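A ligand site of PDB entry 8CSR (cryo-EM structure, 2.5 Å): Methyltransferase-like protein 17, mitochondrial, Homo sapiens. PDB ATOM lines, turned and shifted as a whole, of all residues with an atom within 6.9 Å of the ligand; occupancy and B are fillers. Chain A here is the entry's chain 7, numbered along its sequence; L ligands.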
ATOM      1  N   HIS A 303     -28.823 -21.034 -12.864  1.00  0.00           N
ATOM      2  CA  HIS A 303     -27.701 -20.579 -12.049  1.00  0.00           C
ATOM      3  C   HIS A 303     -26.613 -21.641 -11.964  1.00  0.00           C
ATOM      4  O   HIS A 303     -25.429 -21.323 -12.032  1.00  0.00           O
ATOM      5  CB  HIS A 303     -28.191 -20.180 -10.668  1.00  0.00           C
ATOM      6  CG  HIS A 303     -27.080 -19.845  -9.709  1.00  0.00           C
ATOM      7  ND1 HIS A 303     -26.847 -20.576  -8.566  1.00  0.00           N
ATOM      8  CD2 HIS A 303     -26.138 -18.881  -9.738  1.00  0.00           C
ATOM      9  CE1 HIS A 303     -25.805 -20.062  -7.927  1.00  0.00           C
ATOM     10  NE2 HIS A 303     -25.361 -19.031  -8.616  1.00  0.00           N
ATOM     11  N   MET A 307     -22.541 -21.433 -13.170  1.00  0.00           N
ATOM     12  CA  MET A 307     -21.445 -21.657 -12.225  1.00  0.00           C
ATOM     13  C   MET A 307     -20.519 -22.761 -12.728  1.00  0.00           C
ATOM     14  O   MET A 307     -19.326 -22.764 -12.402  1.00  0.00           O
ATOM     15  CB  MET A 307     -21.994 -21.991 -10.845  1.00  0.00           C
ATOM     16  CG  MET A 307     -22.798 -20.875 -10.174  1.00  0.00           C
ATOM     17  SD  MET A 307     -21.908 -19.334  -9.817  1.00  0.00           S
ATOM     18  CE  MET A 307     -22.091 -18.414 -11.344  1.00  0.00           C
ATOM     19  N   ARG A 310     -18.543 -20.714 -15.098  1.00  0.00           N
ATOM     20  CA  ARG A 310     -17.678 -19.793 -14.362  1.00  0.00           C
ATOM     21  C   ARG A 310     -16.436 -20.503 -13.844  1.00  0.00           C
ATOM     22  O   ARG A 310     -15.324 -19.981 -13.919  1.00  0.00           O
ATOM     23  CB  ARG A 310     -18.442 -19.154 -13.207  1.00  0.00           C
ATOM     24  CG  ARG A 310     -17.636 -18.113 -12.462  1.00  0.00           C
ATOM     25  CD  ARG A 310     -18.451 -17.414 -11.402  1.00  0.00           C
ATOM     26  NE  ARG A 310     -18.351 -18.124 -10.132  1.00  0.00           N
ATOM     27  CZ  ARG A 310     -17.731 -17.688  -9.035  1.00  0.00           C
ATOM     28  NH1 ARG A 310     -17.160 -16.503  -8.986  1.00  0.00           N
ATOM     29  NH2 ARG A 310     -17.683 -18.473  -7.974  1.00  0.00           N
ATOM     30  N   VAL A 329     -13.836 -12.688 -12.943  1.00  0.00           N
ATOM     31  CA  VAL A 329     -15.258 -12.426 -13.027  1.00  0.00           C
ATOM     32  C   VAL A 329     -15.476 -10.919 -12.901  1.00  0.00           C
ATOM     33  O   VAL A 329     -15.274 -10.349 -11.834  1.00  0.00           O
ATOM     34  CB  VAL A 329     -16.042 -13.187 -11.946  1.00  0.00           C
ATOM     35  CG1 VAL A 329     -17.524 -13.110 -12.218  1.00  0.00           C
ATOM     36  CG2 VAL A 329     -15.591 -14.630 -11.899  1.00  0.00           C
ATOM     37  N   ALA A 331     -18.411  -9.403 -13.416  1.00  0.00           N
ATOM     38  CA  ALA A 331     -19.678  -9.249 -12.719  1.00  0.00           C
ATOM     39  C   ALA A 331     -20.442 -10.568 -12.814  1.00  0.00           C
ATOM     40  O   ALA A 331     -20.187 -11.360 -13.726  1.00  0.00           O
ATOM     41  CB  ALA A 331     -20.503  -8.107 -13.306  1.00  0.00           C
ATOM     42  N   PRO A 332     -21.382 -10.826 -11.900  1.00  0.00           N
ATOM     43  CA  PRO A 332     -21.758 -10.025 -10.736  1.00  0.00           C
ATOM     44  C   PRO A 332     -20.959 -10.365  -9.486  1.00  0.00           C
ATOM     45  O   PRO A 332     -21.081  -9.680  -8.478  1.00  0.00           O
ATOM     46  CB  PRO A 332     -23.225 -10.387 -10.545  1.00  0.00           C
ATOM     47  CG  PRO A 332     -23.290 -11.798 -10.965  1.00  0.00           C
ATOM     48  CD  PRO A 332     -22.266 -11.998 -12.044  1.00  0.00           C
ATOM     49  N   CYS A 333     -20.138 -11.399  -9.563  1.00  0.00           N
ATOM     50  CA  CYS A 333     -19.446 -11.868  -8.372  1.00  0.00           C
ATOM     51  C   CYS A 333     -18.280 -10.937  -8.026  1.00  0.00           C
ATOM     52  O   CYS A 333     -17.546 -10.512  -8.916  1.00  0.00           O
ATOM     53  CB  CYS A 333     -18.918 -13.277  -8.581  1.00  0.00           C
ATOM     54  SG  CYS A 333     -20.078 -14.387  -9.378  1.00  0.00           S
ATOM     55  N   PRO A 334     -18.080 -10.587  -6.747  1.00  0.00           N
ATOM     56  CA  PRO A 334     -16.902  -9.787  -6.385  1.00  0.00           C
ATOM     57  C   PRO A 334     -15.683 -10.646  -6.062  1.00  0.00           C
ATOM     58  O   PRO A 334     -14.719 -10.156  -5.472  1.00  0.00           O
ATOM     59  CB  PRO A 334     -17.381  -9.005  -5.161  1.00  0.00           C
ATOM     60  CG  PRO A 334     -18.337  -9.904  -4.517  1.00  0.00           C
ATOM     61  CD  PRO A 334     -19.004 -10.712  -5.600  1.00  0.00           C
ATOM     62  N   HIS A 335     -15.728 -11.921  -6.432  1.00  0.00           N
ATOM     63  CA  HIS A 335     -14.646 -12.847  -6.109  1.00  0.00           C
ATOM     64  C   HIS A 335     -14.620 -13.961  -7.144  1.00  0.00           C
ATOM     65  O   HIS A 335     -15.566 -14.157  -7.911  1.00  0.00           O
ATOM     66  CB  HIS A 335     -14.822 -13.431  -4.706  1.00  0.00           C
ATOM     67  CG  HIS A 335     -16.151 -14.077  -4.498  1.00  0.00           C
ATOM     68  ND1 HIS A 335     -16.433 -15.362  -4.929  1.00  0.00           N
ATOM     69  CD2 HIS A 335     -17.281 -13.629  -3.903  1.00  0.00           C
ATOM     70  CE1 HIS A 335     -17.675 -15.664  -4.615  1.00  0.00           C
ATOM     71  NE2 HIS A 335     -18.212 -14.636  -3.979  1.00  0.00           N
ATOM     72  N   LEU A 337     -13.851 -17.082  -5.900  1.00  0.00           N
ATOM     73  CA  LEU A 337     -14.061 -18.232  -5.037  1.00  0.00           C
ATOM     74  C   LEU A 337     -15.417 -18.846  -5.359  1.00  0.00           C
ATOM     75  O   LEU A 337     -16.263 -18.222  -5.993  1.00  0.00           O
ATOM     76  CB  LEU A 337     -13.989 -17.779  -3.580  1.00  0.00           C
ATOM     77  CG  LEU A 337     -12.638 -17.204  -3.164  1.00  0.00           C
ATOM     78  CD1 LEU A 337     -12.723 -16.611  -1.783  1.00  0.00           C
ATOM     79  CD2 LEU A 337     -11.549 -18.262  -3.224  1.00  0.00           C
ATOM     80  N   PRO A 338     -15.656 -20.104  -4.943  1.00  0.00           N
ATOM     81  CA  PRO A 338     -16.922 -20.757  -5.309  1.00  0.00           C
ATOM     82  C   PRO A 338     -18.137 -19.998  -4.793  1.00  0.00           C
ATOM     83  O   PRO A 338     -18.084 -19.283  -3.803  1.00  0.00           O
ATOM     84  CB  PRO A 338     -16.792 -22.141  -4.648  1.00  0.00           C
ATOM     85  CG  PRO A 338     -15.646 -22.045  -3.727  1.00  0.00           C
ATOM     86  CD  PRO A 338     -14.727 -21.057  -4.331  1.00  0.00           C
ATOM     87  N   CYS A 339     -19.231 -20.160  -5.525  1.00  0.00           N
ATOM     88  CA  CYS A 339     -20.469 -19.463  -5.210  1.00  0.00           C
ATOM     89  C   CYS A 339     -20.985 -19.884  -3.832  1.00  0.00           C
ATOM     90  O   CYS A 339     -21.163 -21.088  -3.588  1.00  0.00           O
ATOM     91  CB  CYS A 339     -21.523 -19.772  -6.267  1.00  0.00           C
ATOM     92  SG  CYS A 339     -23.028 -18.784  -6.179  1.00  0.00           S
ATOM     93  N   PRO A 340     -21.269 -18.947  -2.924  1.00  0.00           N
ATOM     94  CA  PRO A 340     -21.812 -19.346  -1.620  1.00  0.00           C
ATOM     95  C   PRO A 340     -23.306 -19.652  -1.631  1.00  0.00           C
ATOM     96  O   PRO A 340     -23.812 -20.158  -0.622  1.00  0.00           O
ATOM     97  CB  PRO A 340     -21.495 -18.141  -0.734  1.00  0.00           C
ATOM     98  CG  PRO A 340     -21.500 -16.999  -1.656  1.00  0.00           C
ATOM     99  CD  PRO A 340     -20.989 -17.501  -2.966  1.00  0.00           C
ATOM    100  N   GLN A 341     -24.005 -19.374  -2.725  1.00  0.00           N
ATOM    101  CA  GLN A 341     -25.440 -19.631  -2.828  1.00  0.00           C
ATOM    102  C   GLN A 341     -25.759 -20.830  -3.706  1.00  0.00           C
ATOM    103  O   GLN A 341     -26.929 -21.152  -3.902  1.00  0.00           O
ATOM    104  CB  GLN A 341     -26.157 -18.394  -3.379  1.00  0.00           C
ATOM    105  CG  GLN A 341     -26.307 -17.279  -2.381  1.00  0.00           C
ATOM    106  CD  GLN A 341     -27.694 -17.236  -1.761  1.00  0.00           C
ATOM    107  OE1 GLN A 341     -28.626 -16.720  -2.364  1.00  0.00           O
ATOM    108  NE2 GLN A 341     -27.819 -17.777  -0.550  1.00  0.00           N
ATOM    109  N   LEU A 342     -24.749 -21.510  -4.244  1.00  0.00           N
ATOM    110  CA  LEU A 342     -24.989 -22.599  -5.181  1.00  0.00           C
ATOM    111  C   LEU A 342     -25.433 -23.876  -4.492  1.00  0.00           C
ATOM    112  O   LEU A 342     -25.961 -24.762  -5.167  1.00  0.00           O
ATOM    113  CB  LEU A 342     -23.729 -22.864  -6.011  1.00  0.00           C
ATOM    114  CG  LEU A 342     -23.779 -23.937  -7.092  1.00  0.00           C
ATOM    115  CD1 LEU A 342     -24.858 -23.670  -8.119  1.00  0.00           C
ATOM    116  CD2 LEU A 342     -22.417 -24.041  -7.760  1.00  0.00           C
ATOM    117  N   ALA A 346     -30.232 -20.068  -5.289  1.00  0.00           N
ATOM    118  CA  ALA A 346     -29.750 -19.612  -6.585  1.00  0.00           C
ATOM    119  C   ALA A 346     -29.265 -18.179  -6.451  1.00  0.00           C
ATOM    120  O   ALA A 346     -29.206 -17.610  -5.358  1.00  0.00           O
ATOM    121  CB  ALA A 346     -30.843 -19.734  -7.643  1.00  0.00           C
ATOM    122  N   CYS A 347     -28.896 -17.588  -7.578  1.00  0.00           N
ATOM    123  CA  CYS A 347     -28.523 -16.180  -7.650  1.00  0.00           C
ATOM    124  C   CYS A 347     -29.035 -15.622  -8.967  1.00  0.00           C
ATOM    125  O   CYS A 347     -28.583 -16.060 -10.029  1.00  0.00           O
ATOM    126  CB  CYS A 347     -27.009 -15.982  -7.538  1.00  0.00           C
ATOM    127  SG  CYS A 347     -26.482 -14.283  -7.796  1.00  0.00           S
ATOM    128  N   SER A 348     -29.958 -14.684  -8.898  1.00  0.00           N
ATOM    129  CA  SER A 348     -30.585 -14.114 -10.079  1.00  0.00           C
ATOM    130  C   SER A 348     -30.787 -12.626  -9.871  1.00  0.00           C
ATOM    131  O   SER A 348     -30.692 -12.115  -8.751  1.00  0.00           O
ATOM    132  CB  SER A 348     -31.922 -14.801 -10.379  1.00  0.00           C
ATOM    133  OG  SER A 348     -32.760 -14.788  -9.247  1.00  0.00           O
ATOM    134  N   PHE A 349     -31.078 -11.938 -10.966  1.00  0.00           N
ATOM    135  CA  PHE A 349     -31.285 -10.504 -10.961  1.00  0.00           C
ATOM    136  C   PHE A 349     -32.514 -10.201 -11.799  1.00  0.00           C
ATOM    137  O   PHE A 349     -32.987 -11.048 -12.558  1.00  0.00           O
ATOM    138  CB  PHE A 349     -30.046  -9.776 -11.494  1.00  0.00           C
ATOM    139  CG  PHE A 349     -28.830  -9.990 -10.664  1.00  0.00           C
ATOM    140  CD1 PHE A 349     -28.601  -9.242  -9.525  1.00  0.00           C
ATOM    141  CD2 PHE A 349     -27.917 -10.975 -10.993  1.00  0.00           C
ATOM    142  CE1 PHE A 349     -27.484  -9.447  -8.759  1.00  0.00           C
ATOM    143  CE2 PHE A 349     -26.790 -11.181 -10.237  1.00  0.00           C
ATOM    144  CZ  PHE A 349     -26.580 -10.419  -9.100  1.00  0.00           C
ATOM    145  N   MET A 371     -26.718 -14.166 -14.651  1.00  0.00           N
ATOM    146  CA  MET A 371     -25.658 -13.681 -15.528  1.00  0.00           C
ATOM    147  C   MET A 371     -24.314 -13.910 -14.881  1.00  0.00           C
ATOM    148  O   MET A 371     -24.179 -13.948 -13.657  1.00  0.00           O
ATOM    149  CB  MET A 371     -25.855 -12.186 -15.865  1.00  0.00           C
ATOM    150  CG  MET A 371     -25.383 -11.173 -14.825  1.00  0.00           C
ATOM    151  SD  MET A 371     -25.186  -9.512 -15.488  1.00  0.00           S
ATOM    152  CE  MET A 371     -24.113  -8.790 -14.262  1.00  0.00           C
ATOM    153  N   VAL A 372     -23.298 -14.066 -15.738  1.00  0.00           N
ATOM    154  CA  VAL A 372     -21.902 -14.024 -15.320  1.00  0.00           C
ATOM    155  C   VAL A 372     -21.107 -13.423 -16.466  1.00  0.00           C
ATOM    156  O   VAL A 372     -21.290 -13.798 -17.619  1.00  0.00           O
ATOM    157  CB  VAL A 372     -21.366 -15.414 -14.913  1.00  0.00           C
ATOM    158  CG1 VAL A 372     -21.357 -16.356 -16.099  1.00  0.00           C
ATOM    159  CG2 VAL A 372     -19.969 -15.283 -14.332  1.00  0.00           C
ATOM    160  N   ARG A 387     -22.016  -7.138  -3.710  1.00  0.00           N
ATOM    161  CA  ARG A 387     -23.117  -7.112  -4.667  1.00  0.00           C
ATOM    162  C   ARG A 387     -24.414  -7.444  -3.941  1.00  0.00           C
ATOM    163  O   ARG A 387     -24.488  -8.451  -3.229  1.00  0.00           O
ATOM    164  CB  ARG A 387     -22.854  -8.105  -5.804  1.00  0.00           C
ATOM    165  CG  ARG A 387     -24.030  -8.395  -6.746  1.00  0.00           C
ATOM    166  CD  ARG A 387     -24.159  -7.388  -7.869  1.00  0.00           C
ATOM    167  NE  ARG A 387     -22.958  -7.257  -8.673  1.00  0.00           N
ATOM    168  CZ  ARG A 387     -22.836  -6.464  -9.723  1.00  0.00           C
ATOM    169  NH1 ARG A 387     -23.845  -5.725 -10.156  1.00  0.00           N
ATOM    170  NH2 ARG A 387     -21.673  -6.391 -10.361  1.00  0.00           N
ATOM    171  N   THR A 389     -27.750  -9.042  -4.052  1.00  0.00           N
ATOM    172  CA  THR A 389     -28.221 -10.130  -4.891  1.00  0.00           C
ATOM    173  C   THR A 389     -29.691 -10.449  -4.669  1.00  0.00           C
ATOM    174  O   THR A 389     -30.148 -11.520  -5.083  1.00  0.00           O
ATOM    175  CB  THR A 389     -27.396 -11.384  -4.627  1.00  0.00           C
ATOM    176  OG1 THR A 389     -27.600 -11.824  -3.279  1.00  0.00           O
ATOM    177  CG2 THR A 389     -25.920 -11.106  -4.815  1.00  0.00           C
ATOM    178  N   LEU A 403     -25.934  -9.362   0.789  1.00  0.00           N
ATOM    179  CA  LEU A 403     -24.734  -9.027   0.042  1.00  0.00           C
ATOM    180  C   LEU A 403     -23.853 -10.252  -0.156  1.00  0.00           C
ATOM    181  O   LEU A 403     -23.622 -11.024   0.776  1.00  0.00           O
ATOM    182  CB  LEU A 403     -23.911  -7.959   0.770  1.00  0.00           C
ATOM    183  CG  LEU A 403     -24.626  -6.643   1.056  1.00  0.00           C
ATOM    184  CD1 LEU A 403     -24.037  -6.015   2.304  1.00  0.00           C
ATOM    185  CD2 LEU A 403     -24.538  -5.704  -0.126  1.00  0.00           C
ATOM    186  N   CYS A 404     -23.369 -10.415  -1.377  1.00  0.00           N
ATOM    187  CA  CYS A 404     -22.281 -11.328  -1.679  1.00  0.00           C
ATOM    188  C   CYS A 404     -20.980 -10.541  -1.528  1.00  0.00           C
ATOM    189  O   CYS A 404     -20.717  -9.611  -2.286  1.00  0.00           O
ATOM    190  CB  CYS A 404     -22.416 -11.904  -3.089  1.00  0.00           C
ATOM    191  SG  CYS A 404     -21.280 -13.228  -3.509  1.00  0.00           S
ATOM    192  N   CYS A 405     -20.182 -10.900  -0.533  1.00  0.00           N
ATOM    193  CA  CYS A 405     -19.027 -10.096  -0.166  1.00  0.00           C
ATOM    194  C   CYS A 405     -17.784 -10.532  -0.903  1.00  0.00           C
ATOM    195  O   CYS A 405     -17.718 -11.661  -1.418  1.00  0.00           O
ATOM    196  CB  CYS A 405     -18.798 -10.176   1.340  1.00  0.00           C
ATOM    197  SG  CYS A 405     -20.289  -9.869   2.312  1.00  0.00           S
ATOM    198  N   GLY A 408     -16.037 -14.072  -0.305  1.00  0.00           N
ATOM    199  CA  GLY A 408     -16.650 -15.311  -0.731  1.00  0.00           C
ATOM    200  C   GLY A 408     -17.831 -15.766   0.087  1.00  0.00           C
ATOM    201  O   GLY A 408     -18.272 -16.903  -0.092  1.00  0.00           O
ATOM    202  N   MET A 410     -21.807 -14.806   1.910  1.00  0.00           N
ATOM    203  CA  MET A 410     -22.978 -13.946   1.968  1.00  0.00           C
ATOM    204  C   MET A 410     -23.116 -13.321   3.341  1.00  0.00           C
ATOM    205  O   MET A 410     -22.739 -13.924   4.346  1.00  0.00           O
ATOM    206  CB  MET A 410     -24.248 -14.715   1.629  1.00  0.00           C
ATOM    207  CG  MET A 410     -24.189 -15.560   0.376  1.00  0.00           C
ATOM    208  SD  MET A 410     -24.268 -14.527  -1.091  1.00  0.00           S
ATOM    209  CE  MET A 410     -26.027 -14.249  -1.213  1.00  0.00           C
HETATM  210 FE1  LIG L   1     -22.361 -14.121  -5.282  1.00  0.00          FE
HETATM  211 FE2  LIG L   1     -24.322 -14.522  -7.208  1.00  0.00          FE
HETATM  212 FE3  LIG L   1     -21.735 -14.583  -7.874  1.00  0.00          FE
HETATM  213 FE4  LIG L   1     -22.778 -16.557  -6.364  1.00  0.00          FE
HETATM  214  S1  LIG L   1     -23.382 -16.060  -8.511  1.00  0.00           S
HETATM  215  S2  LIG L   1     -20.773 -15.511  -5.991  1.00  0.00           S
HETATM  216  S3  LIG L   1     -24.264 -15.420  -5.092  1.00  0.00           S
HETATM  217  S4  LIG L   1     -22.820 -12.780  -7.088  1.00  0.00           S
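The side-chain sulfur (SG) of Cys 339 is bound to an iron atom (FE4) of the ligand, 2.2 Å away. An iron atom (FE2) of the ligand is bound by the side-chain sulfur (SG) of Cys 347 (2.3 Å). A ring nitrogen (NE2) of His 303 lies close to a sulfur (S1) of the ligand, at 3.6 Å. The side-chain sulfur of Cys 404 binds an iron atom (FE1) of the ligand, 2.3 Å away. A ring nitrogen (NE2) of His 335 sits close to a sulfur (S2) of the ligand (3.4 Å). SG of Cys 333 is bound to FE3 of the ligand.
The backbone carbonyl oxygen of His 335 is in hydrogen-bond range of the guanidinium group of Arg 310. The guanidinium group (NE) of Arg 387 is in hydrogen-bond range of the backbone carbonyl oxygen (O) of Pro 332, at 3.1 Å. The side-chain sulfur of Cys 339 lies close to the backbone NH of Leu 342, at 3.8 Å. The backbone NH (N) of Cys 404 lies within hydrogen-bond range of the backbone carbonyl oxygen (O) of Arg 387 (2.9 Å). NE2 of His 303 sits close to SD of Met 307, 3.7 Å away. The guanidinium group of Arg 310 lies within hydrogen-bond range of the side-chain sulfur of Met 307. A ring nitrogen (NE2) of His 303 sits close to the side-chain sulfur (SG) of Cys 339 (3.4 Å). A ring nitrogen (ND1) of His 335 sits at hydrogen-bond distance from the backbone carbonyl oxygen (O) of Leu 337 (3.1 Å).
Met 307 touches the ligand (SD to S1, 3.8 Å). O of Pro 332 touches S4 of the ligand, 3.8 Å away. Pro 340 touches the ligand. Gln 341 touches the ligand. Hydrophobic or aromatic side chains within 4 Å of the ligand: Met 307, His 335 and Pro 340.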
